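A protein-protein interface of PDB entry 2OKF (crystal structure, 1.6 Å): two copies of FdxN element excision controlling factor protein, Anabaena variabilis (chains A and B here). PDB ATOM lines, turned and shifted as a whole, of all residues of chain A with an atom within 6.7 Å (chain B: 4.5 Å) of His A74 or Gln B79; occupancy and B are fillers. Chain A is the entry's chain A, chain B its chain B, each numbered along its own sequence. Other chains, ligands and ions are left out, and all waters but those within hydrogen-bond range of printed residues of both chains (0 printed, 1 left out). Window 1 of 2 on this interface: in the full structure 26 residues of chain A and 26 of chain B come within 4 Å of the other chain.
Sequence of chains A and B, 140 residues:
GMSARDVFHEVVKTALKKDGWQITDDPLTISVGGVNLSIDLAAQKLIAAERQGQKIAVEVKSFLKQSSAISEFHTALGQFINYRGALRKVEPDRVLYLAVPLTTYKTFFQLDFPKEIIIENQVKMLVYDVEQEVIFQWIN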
ATOM      1  N   PHE A  63     -16.430  -1.646 -12.854  1.00  0.00           N
ATOM      2  CA  PHE A  63     -15.448  -1.594 -11.783  1.00  0.00           C
ATOM      3  C   PHE A  63     -16.114  -1.519 -10.419  1.00  0.00           C
ATOM      4  O   PHE A  63     -15.903  -0.587  -9.642  1.00  0.00           O
ATOM      5  CB  PHE A  63     -14.436  -0.454 -12.010  1.00  0.00           C
ATOM      6  CG  PHE A  63     -13.393  -0.790 -13.040  1.00  0.00           C
ATOM      7  CD1 PHE A  63     -12.229  -1.439 -12.668  1.00  0.00           C
ATOM      8  CD2 PHE A  63     -13.590  -0.491 -14.369  1.00  0.00           C
ATOM      9  CE1 PHE A  63     -11.285  -1.774 -13.609  1.00  0.00           C
ATOM     10  CE2 PHE A  63     -12.638  -0.841 -15.318  1.00  0.00           C
ATOM     11  CZ  PHE A  63     -11.488  -1.479 -14.924  1.00  0.00           C
ATOM     12  N   SER A  68     -11.337  -6.562  -6.447  1.00  0.00           N
ATOM     13  CA  SER A  68     -10.314  -5.552  -6.512  1.00  0.00           C
ATOM     14  C   SER A  68     -10.385  -4.895  -7.866  1.00  0.00           C
ATOM     15  O   SER A  68     -10.686  -5.566  -8.887  1.00  0.00           O
ATOM     16  CB  SER A  68      -8.934  -6.145  -6.289  1.00  0.00           C
ATOM     17  OG  SER A  68      -8.621  -7.112  -7.274  1.00  0.00           O
ATOM     18  N   ALA A  69     -10.118  -3.585  -7.893  1.00  0.00           N
ATOM     19  CA  ALA A  69     -10.051  -2.883  -9.151  1.00  0.00           C
ATOM     20  C   ALA A  69      -8.948  -3.510 -10.009  1.00  0.00           C
ATOM     21  O   ALA A  69      -9.130  -3.668 -11.213  1.00  0.00           O
ATOM     22  CB  ALA A  69      -9.796  -1.387  -8.924  1.00  0.00           C
ATOM     23  N   ILE A  70      -7.832  -3.909  -9.385  1.00  0.00           N
ATOM     24  CA  ILE A  70      -6.729  -4.501 -10.154  1.00  0.00           C
ATOM     25  C   ILE A  70      -7.169  -5.831 -10.819  1.00  0.00           C
ATOM     26  O   ILE A  70      -6.856  -6.078 -11.974  1.00  0.00           O
ATOM     27  CB  ILE A  70      -5.396  -4.613  -9.368  1.00  0.00           C
ATOM     28  CG1 ILE A  70      -4.258  -5.098 -10.268  1.00  0.00           C
ATOM     29  CG2 ILE A  70      -5.523  -5.545  -8.202  1.00  0.00           C
ATOM     30  CD1 ILE A  70      -3.912  -4.166 -11.440  1.00  0.00           C
ATOM     31  N   SER A  71      -7.899  -6.684 -10.112  1.00  0.00           N
ATOM     32  CA  SER A  71      -8.352  -7.931 -10.730  1.00  0.00           C
ATOM     33  C   SER A  71      -9.293  -7.643 -11.904  1.00  0.00           C
ATOM     34  O   SER A  71      -9.209  -8.290 -12.970  1.00  0.00           O
ATOM     35  CB  SER A  71      -9.066  -8.832  -9.723  1.00  0.00           C
ATOM     36  OG  SER A  71     -10.218  -8.239  -9.255  1.00  0.00           O
ATOM     37  N   GLU A  72     -10.185  -6.672 -11.718  1.00  0.00           N
ATOM     38  CA  GLU A  72     -11.124  -6.273 -12.765  1.00  0.00           C
ATOM     39  C   GLU A  72     -10.347  -5.726 -13.934  1.00  0.00           C
ATOM     40  O   GLU A  72     -10.689  -5.975 -15.102  1.00  0.00           O
ATOM     41  CB  GLU A  72     -12.084  -5.217 -12.218  1.00  0.00           C
ATOM     42  CG  GLU A  72     -12.962  -5.760 -11.157  1.00  0.00           C
ATOM     43  CD  GLU A  72     -13.652  -4.719 -10.261  1.00  0.00           C
ATOM     44  OE1 GLU A  72     -13.290  -3.524 -10.249  1.00  0.00           O
ATOM     45  OE2 GLU A  72     -14.585  -5.140  -9.551  1.00  0.00           O
ATOM     46  N   PHE A  73      -9.294  -4.973 -13.640  1.00  0.00           N
ATOM     47  CA  PHE A  73      -8.452  -4.384 -14.660  1.00  0.00           C
ATOM     48  C   PHE A  73      -7.710  -5.434 -15.461  1.00  0.00           C
ATOM     49  O   PHE A  73      -7.639  -5.304 -16.675  1.00  0.00           O
ATOM     50  CB  PHE A  73      -7.516  -3.309 -14.074  1.00  0.00           C
ATOM     51  CG  PHE A  73      -6.679  -2.587 -15.101  1.00  0.00           C
ATOM     52  CD1 PHE A  73      -7.265  -2.000 -16.207  1.00  0.00           C
ATOM     53  CD2 PHE A  73      -5.289  -2.480 -14.953  1.00  0.00           C
ATOM     54  CE1 PHE A  73      -6.457  -1.356 -17.181  1.00  0.00           C
ATOM     55  CE2 PHE A  73      -4.534  -1.764 -15.858  1.00  0.00           C
ATOM     56  CZ  PHE A  73      -5.110  -1.222 -16.962  1.00  0.00           C
ATOM     57  N   HIS A  74      -7.149  -6.451 -14.813  1.00  0.00           N
ATOM     58  CA  HIS A  74      -6.481  -7.507 -15.580  1.00  0.00           C
ATOM     59  C   HIS A  74      -7.412  -8.054 -16.688  1.00  0.00           C
ATOM     60  O   HIS A  74      -7.049  -8.186 -17.846  1.00  0.00           O
ATOM     61  CB  HIS A  74      -6.079  -8.710 -14.726  1.00  0.00           C
ATOM     62  CG  HIS A  74      -5.034  -8.434 -13.709  1.00  0.00           C
ATOM     63  ND1 HIS A  74      -3.887  -7.717 -13.995  1.00  0.00           N
ATOM     64  CD2 HIS A  74      -4.919  -8.862 -12.427  1.00  0.00           C
ATOM     65  CE1 HIS A  74      -3.124  -7.709 -12.907  1.00  0.00           C
ATOM     66  NE2 HIS A  74      -3.712  -8.414 -11.952  1.00  0.00           N
ATOM     67  N   THR A  75      -8.614  -8.444 -16.289  1.00  0.00           N
ATOM     68  CA  THR A  75      -9.548  -9.024 -17.252  1.00  0.00           C
ATOM     69  C   THR A  75      -9.967  -8.000 -18.306  1.00  0.00           C
ATOM     70  O   THR A  75      -9.988  -8.282 -19.512  1.00  0.00           O
ATOM     71  CB  THR A  75     -10.742  -9.610 -16.540  1.00  0.00           C
ATOM     72  OG1 THR A  75     -10.295 -10.654 -15.669  1.00  0.00           O
ATOM     73  CG2 THR A  75     -11.739 -10.180 -17.542  1.00  0.00           C
ATOM     74  N   ALA A  76     -10.279  -6.773 -17.872  1.00  0.00           N
ATOM     75  CA  ALA A  76     -10.666  -5.726 -18.822  1.00  0.00           C
ATOM     76  C   ALA A  76      -9.573  -5.447 -19.862  1.00  0.00           C
ATOM     77  O   ALA A  76      -9.867  -5.205 -21.032  1.00  0.00           O
ATOM     78  CB  ALA A  76     -11.024  -4.429 -18.112  1.00  0.00           C
ATOM     79  N   LEU A  77      -8.327  -5.426 -19.398  1.00  0.00           N
ATOM     80  CA  LEU A  77      -7.185  -5.146 -20.259  1.00  0.00           C
ATOM     81  C   LEU A  77      -6.983  -6.289 -21.274  1.00  0.00           C
ATOM     82  O   LEU A  77      -6.742  -6.052 -22.456  1.00  0.00           O
ATOM     83  CB  LEU A  77      -5.923  -4.941 -19.420  1.00  0.00           C
ATOM     84  CG  LEU A  77      -4.658  -4.638 -20.200  1.00  0.00           C
ATOM     85  CD1 LEU A  77      -4.746  -3.348 -21.069  1.00  0.00           C
ATOM     86  CD2 LEU A  77      -3.510  -4.588 -19.205  1.00  0.00           C
ATOM     87  N   GLY A  78      -7.018  -7.526 -20.795  1.00  0.00           N
ATOM     88  CA  GLY A  78      -6.867  -8.675 -21.677  1.00  0.00           C
ATOM     89  C   GLY A  78      -7.950  -8.721 -22.733  1.00  0.00           C
ATOM     90  O   GLY A  78      -7.679  -8.950 -23.915  1.00  0.00           O
ATOM     91  N   GLN A  79      -9.187  -8.493 -22.290  1.00  0.00           N
ATOM     92  CA  GLN A  79     -10.304  -8.397 -23.226  1.00  0.00           C
ATOM     93  C   GLN A  79     -10.055  -7.284 -24.252  1.00  0.00           C
ATOM     94  O   GLN A  79     -10.253  -7.470 -25.464  1.00  0.00           O
ATOM     95  CB  GLN A  79     -11.631  -8.199 -22.471  1.00  0.00           C
ATOM     96  CG  GLN A  79     -12.081  -9.446 -21.696  1.00  0.00           C
ATOM     97  CD  GLN A  79     -13.206  -9.203 -20.700  1.00  0.00           C
ATOM     98  OE1 GLN A  79     -13.434  -8.081 -20.261  1.00  0.00           O
ATOM     99  NE2 GLN A  79     -13.870 -10.291 -20.286  1.00  0.00           N
ATOM    100  N   PHE A 113       0.384   3.507 -11.644  1.00  0.00           N
ATOM    101  CA  PHE A 113       0.527   2.260 -12.414  1.00  0.00           C
ATOM    102  C   PHE A 113      -0.557   2.084 -13.491  1.00  0.00           C
ATOM    103  O   PHE A 113      -0.237   1.892 -14.669  1.00  0.00           O
ATOM    104  CB  PHE A 113       0.652   1.062 -11.491  1.00  0.00           C
ATOM    105  CG  PHE A 113       0.656  -0.238 -12.224  1.00  0.00           C
ATOM    106  CD1 PHE A 113       1.786  -0.656 -12.856  1.00  0.00           C
ATOM    107  CD2 PHE A 113      -0.512  -0.959 -12.377  1.00  0.00           C
ATOM    108  CE1 PHE A 113       1.780  -1.841 -13.557  1.00  0.00           C
ATOM    109  CE2 PHE A 113      -0.516  -2.148 -13.107  1.00  0.00           C
ATOM    110  CZ  PHE A 113       0.614  -2.559 -13.690  1.00  0.00           C
ATOM    111  N   LEU B  37      -0.034  -5.713  -6.797  1.00  0.00           N
ATOM    112  CA  LEU B  37      -0.487  -6.751  -7.705  1.00  0.00           C
ATOM    113  C   LEU B  37      -0.389  -8.120  -7.044  1.00  0.00           C
ATOM    114  O   LEU B  37      -0.223  -8.205  -5.820  1.00  0.00           O
ATOM    115  CB  LEU B  37       0.317  -6.708  -9.009  1.00  0.00           C
ATOM    116  CG  LEU B  37       0.095  -5.478  -9.894  1.00  0.00           C
ATOM    117  CD1 LEU B  37       0.906  -4.294  -9.400  1.00  0.00           C
ATOM    118  CD2 LEU B  37       0.501  -5.778 -11.319  1.00  0.00           C
ATOM    119  N   GLU B  59       4.106 -16.770 -14.629  1.00  0.00           N
ATOM    120  CA  GLU B  59       2.650 -16.685 -14.475  1.00  0.00           C
ATOM    121  C   GLU B  59       2.035 -18.036 -14.841  1.00  0.00           C
ATOM    122  O   GLU B  59       2.047 -18.429 -15.978  1.00  0.00           O
ATOM    123  CB  GLU B  59       2.083 -15.572 -15.343  1.00  0.00           C
ATOM    124  CG  GLU B  59       0.566 -15.529 -15.389  1.00  0.00           C
ATOM    125  CD  GLU B  59       0.049 -14.535 -16.359  1.00  0.00           C
ATOM    126  OE1 GLU B  59       0.784 -13.601 -16.723  1.00  0.00           O
ATOM    127  OE2 GLU B  59      -1.146 -14.665 -16.778  1.00  0.00           O
ATOM    128  N   LYS B  61      -0.687 -20.849 -15.508  1.00  0.00           N
ATOM    129  CA  LYS B  61      -2.060 -21.114 -15.952  1.00  0.00           C
ATOM    130  C   LYS B  61      -2.225 -22.603 -16.274  1.00  0.00           C
ATOM    131  O   LYS B  61      -1.274 -23.290 -16.728  1.00  0.00           O
ATOM    132  CB  LYS B  61      -2.436 -20.251 -17.159  1.00  0.00           C
ATOM    133  CG  LYS B  61      -2.372 -18.766 -16.827  1.00  0.00           C
ATOM    134  CD  LYS B  61      -3.478 -18.393 -15.867  1.00  0.00           C
ATOM    135  CE  LYS B  61      -3.363 -16.989 -15.378  1.00  0.00           C
ATOM    136  NZ  LYS B  61      -4.542 -16.594 -14.550  1.00  0.00           N
ATOM    137  N   HIS B  74      -8.239 -14.215 -21.833  1.00  0.00           N
ATOM    138  CA  HIS B  74      -8.367 -12.774 -21.571  1.00  0.00           C
ATOM    139  C   HIS B  74      -7.681 -12.379 -20.252  1.00  0.00           C
ATOM    140  O   HIS B  74      -6.915 -11.437 -20.164  1.00  0.00           O
ATOM    141  CB  HIS B  74      -9.822 -12.321 -21.426  1.00  0.00           C
ATOM    142  CG  HIS B  74     -10.626 -12.407 -22.666  1.00  0.00           C
ATOM    143  ND1 HIS B  74     -10.141 -12.015 -23.902  1.00  0.00           N
ATOM    144  CD2 HIS B  74     -11.915 -12.777 -22.858  1.00  0.00           C
ATOM    145  CE1 HIS B  74     -11.110 -12.141 -24.796  1.00  0.00           C
ATOM    146  NE2 HIS B  74     -12.204 -12.584 -24.190  1.00  0.00           N
ATOM    147  N   THR B  75      -8.041 -13.084 -19.189  1.00  0.00           N
ATOM    148  CA  THR B  75      -7.484 -12.763 -17.872  1.00  0.00           C
ATOM    149  C   THR B  75      -5.985 -13.024 -17.834  1.00  0.00           C
ATOM    150  O   THR B  75      -5.189 -12.215 -17.330  1.00  0.00           O
ATOM    151  CB  THR B  75      -8.187 -13.547 -16.790  1.00  0.00           C
ATOM    152  OG1 THR B  75      -9.573 -13.179 -16.783  1.00  0.00           O
ATOM    153  CG2 THR B  75      -7.597 -13.220 -15.422  1.00  0.00           C
ATOM    154  N   ALA B  76      -5.549 -14.156 -18.369  1.00  0.00           N
ATOM    155  CA  ALA B  76      -4.122 -14.484 -18.398  1.00  0.00           C
ATOM    156  C   ALA B  76      -3.296 -13.429 -19.155  1.00  0.00           C
ATOM    157  O   ALA B  76      -2.181 -13.089 -18.750  1.00  0.00           O
ATOM    158  CB  ALA B  76      -3.876 -15.841 -19.038  1.00  0.00           C
ATOM    159  N   LEU B  77      -3.839 -12.956 -20.273  1.00  0.00           N
ATOM    160  CA  LEU B  77      -3.186 -11.953 -21.113  1.00  0.00           C
ATOM    161  C   LEU B  77      -3.077 -10.621 -20.372  1.00  0.00           C
ATOM    162  O   LEU B  77      -2.058  -9.957 -20.401  1.00  0.00           O
ATOM    163  CB  LEU B  77      -3.923 -11.784 -22.419  1.00  0.00           C
ATOM    164  CG  LEU B  77      -3.316 -10.785 -23.404  1.00  0.00           C
ATOM    165  CD1 LEU B  77      -1.856 -11.080 -23.783  1.00  0.00           C
ATOM    166  CD2 LEU B  77      -4.216 -10.665 -24.591  1.00  0.00           C
ATOM    167  N   GLY B  78      -4.176 -10.191 -19.779  1.00  0.00           N
ATOM    168  CA  GLY B  78      -4.194  -8.922 -19.041  1.00  0.00           C
ATOM    169  C   GLY B  78      -3.221  -8.962 -17.870  1.00  0.00           C
ATOM    170  O   GLY B  78      -2.485  -8.000 -17.630  1.00  0.00           O
ATOM    171  N   GLN B  79      -3.259 -10.061 -17.132  1.00  0.00           N
ATOM    172  CA  GLN B  79      -2.286 -10.270 -16.055  1.00  0.00           C
ATOM    173  C   GLN B  79      -0.866 -10.183 -16.607  1.00  0.00           C
ATOM    174  O   GLN B  79       0.016  -9.534 -16.025  1.00  0.00           O
ATOM    175  CB  GLN B  79      -2.525 -11.595 -15.315  1.00  0.00           C
ATOM    176  CG  GLN B  79      -3.750 -11.596 -14.466  1.00  0.00           C
ATOM    177  CD  GLN B  79      -4.134 -12.963 -13.907  1.00  0.00           C
ATOM    178  OE1 GLN B  79      -3.737 -13.977 -14.441  1.00  0.00           O
ATOM    179  NE2 GLN B  79      -4.997 -12.970 -12.896  1.00  0.00           N
ATOM    180  N   PHE B  80      -0.594 -10.852 -17.712  1.00  0.00           N
ATOM    181  CA  PHE B  80       0.740 -10.859 -18.286  1.00  0.00           C
ATOM    182  C   PHE B  80       1.202  -9.452 -18.603  1.00  0.00           C
ATOM    183  O   PHE B  80       2.320  -9.063 -18.271  1.00  0.00           O
ATOM    184  CB  PHE B  80       0.792 -11.758 -19.534  1.00  0.00           C
ATOM    185  CG  PHE B  80       2.154 -11.867 -20.119  1.00  0.00           C
ATOM    186  CD1 PHE B  80       2.636 -10.929 -21.012  1.00  0.00           C
ATOM    187  CD2 PHE B  80       3.030 -12.875 -19.701  1.00  0.00           C
ATOM    188  CE1 PHE B  80       3.894 -11.030 -21.488  1.00  0.00           C
ATOM    189  CE2 PHE B  80       4.294 -12.951 -20.210  1.00  0.00           C
ATOM    190  CZ  PHE B  80       4.744 -12.025 -21.085  1.00  0.00           C
ATOM    191  N   ILE B  81       0.366  -8.675 -19.294  1.00  0.00           N
ATOM    192  CA  ILE B  81       0.743  -7.325 -19.668  1.00  0.00           C
ATOM    193  C   ILE B  81       0.955  -6.455 -18.432  1.00  0.00           C
ATOM    194  O   ILE B  81       1.935  -5.711 -18.358  1.00  0.00           O
ATOM    195  CB  ILE B  81      -0.329  -6.740 -20.637  1.00  0.00           C
ATOM    196  CG1 ILE B  81      -0.263  -7.524 -21.957  1.00  0.00           C
ATOM    197  CG2 ILE B  81      -0.096  -5.227 -20.858  1.00  0.00           C
ATOM    198  CD1 ILE B  81      -1.329  -7.187 -22.905  1.00  0.00           C
ATOM    199  N   ASN B  82       0.070  -6.563 -17.430  1.00  0.00           N
ATOM    200  CA  ASN B  82       0.223  -5.791 -16.205  1.00  0.00           C
ATOM    201  C   ASN B  82       1.465  -6.175 -15.441  1.00  0.00           C
ATOM    202  O   ASN B  82       2.238  -5.307 -15.023  1.00  0.00           O
ATOM    203  CB  ASN B  82      -1.016  -5.889 -15.323  1.00  0.00           C
ATOM    204  CG  ASN B  82      -2.109  -4.946 -15.774  1.00  0.00           C
ATOM    205  OD1 ASN B  82      -1.818  -3.886 -16.257  1.00  0.00           O
ATOM    206  ND2 ASN B  82      -3.343  -5.320 -15.651  1.00  0.00           N
ATOM    207  N   TYR B  83       1.679  -7.466 -15.259  1.00  0.00           N
ATOM    208  CA  TYR B  83       2.885  -7.936 -14.539  1.00  0.00           C
ATOM    209  C   TYR B  83       4.144  -7.576 -15.278  1.00  0.00           C
ATOM    210  O   TYR B  83       5.128  -7.155 -14.643  1.00  0.00           O
ATOM    211  CB  TYR B  83       2.835  -9.435 -14.256  1.00  0.00           C
ATOM    212  CG  TYR B  83       1.688  -9.916 -13.391  1.00  0.00           C
ATOM    213  CD1 TYR B  83       1.125  -9.119 -12.426  1.00  0.00           C
ATOM    214  CD2 TYR B  83       1.195 -11.182 -13.571  1.00  0.00           C
ATOM    215  CE1 TYR B  83       0.055  -9.575 -11.643  1.00  0.00           C
ATOM    216  CE2 TYR B  83       0.161 -11.670 -12.783  1.00  0.00           C
ATOM    217  CZ  TYR B  83      -0.409 -10.858 -11.833  1.00  0.00           C
ATOM    218  OH  TYR B  83      -1.486 -11.269 -11.061  1.00  0.00           O
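Hydrophobic or aromatic side chains of chain A within 4 Å of the printed part of chain B: Phe A73, His A74, Leu A77 and Phe A113.
Along chain A the printed residues that touch a printed residue of chain B span positions 73 to 113.
Hydrophobic or aromatic side chains of chain B that line the printed part of chain A: Leu B37, His B74, Leu B77, Ile B81 and Tyr B83.
Along chain B the printed residues that touch a printed residue of chain A span positions 37 to 83.
Among the printed residues, 16 pairs touch across the chains.
Among the printed residues, merely in contact across the chains: Phe A73 with Asn B82 (3.5 Å), His A74 with His B74 (3.995 Å), His A74 with Gly B78 (3.2 Å), His A74 with Gln B79 (3.5 Å), His A74 with Tyr B83 (3.7 Å), Leu A77 with Gly B78 (3.9 Å), Leu A77 with Ile B81 (3.8 Å), Leu A77 with Asn B82 (3.5 Å), Gly A78 with His B74 (3.1 Å), Gly A78 with Leu B77 (3.9 Å), Gly A78 with Gly B78 (3.6 Å), Gln A79 with His B74 (3.4 Å), Phe A113 with Leu B37 (3.9995 Å) and Phe A113 with Asn B82 (3.5 Å).
Printed residues of chain B within 4 Å of Phe A73: Asn B82 (3.5 Å).
Of the printed residues of chain B, His A74 touches His B74 (3.995 Å), Gly B78 (3.2 Å), Gln B79 (3.5 Å), Asn B82 (3.0 Å) and Tyr B83 (3.7 Å).
Printed residues of chain A within 4 Å of His B74: His A74, Gly A78 and Gln A79.
Printed residues of chain A within 4 Å of Gly B78: His A74, Leu A77 and Gly A78.
Gln B79 touches one residue of chain A.
The nearest printed residue of chain A that does not touch Leu B37 is Ile A70 (4.4 Å).
The side-chain amide nitrogen (ND2) of Asn B82 sits at hydrogen-bond distance from the backbone carbonyl oxygen (O) of Gly B78.
The side-chain amino group (NZ) of Lys B61 is in hydrogen-bond range of the side-chain amide oxygen (OE1) of Gln B79.
His A74 touches its own counterpart, His B74.
His A74 touches Gly B78, and with the chains exchanged Gly A78 touches His B74.
Thr B75 touches its own counterpart, Thr A75.
Gly A78 touches its own counterpart, Gly B78.
Of the 16 pairs that touch across the chains among the printed residues, 9 have their exchanged pair printed and touching as well.
OG1 of Thr A75 lies within hydrogen-bond range of OG1 of Thr B75 (2.9 Å).
A ring nitrogen (ND1) of His A74 sits at hydrogen-bond distance from the side-chain amide nitrogen of Asn B82 (3.0 Å).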
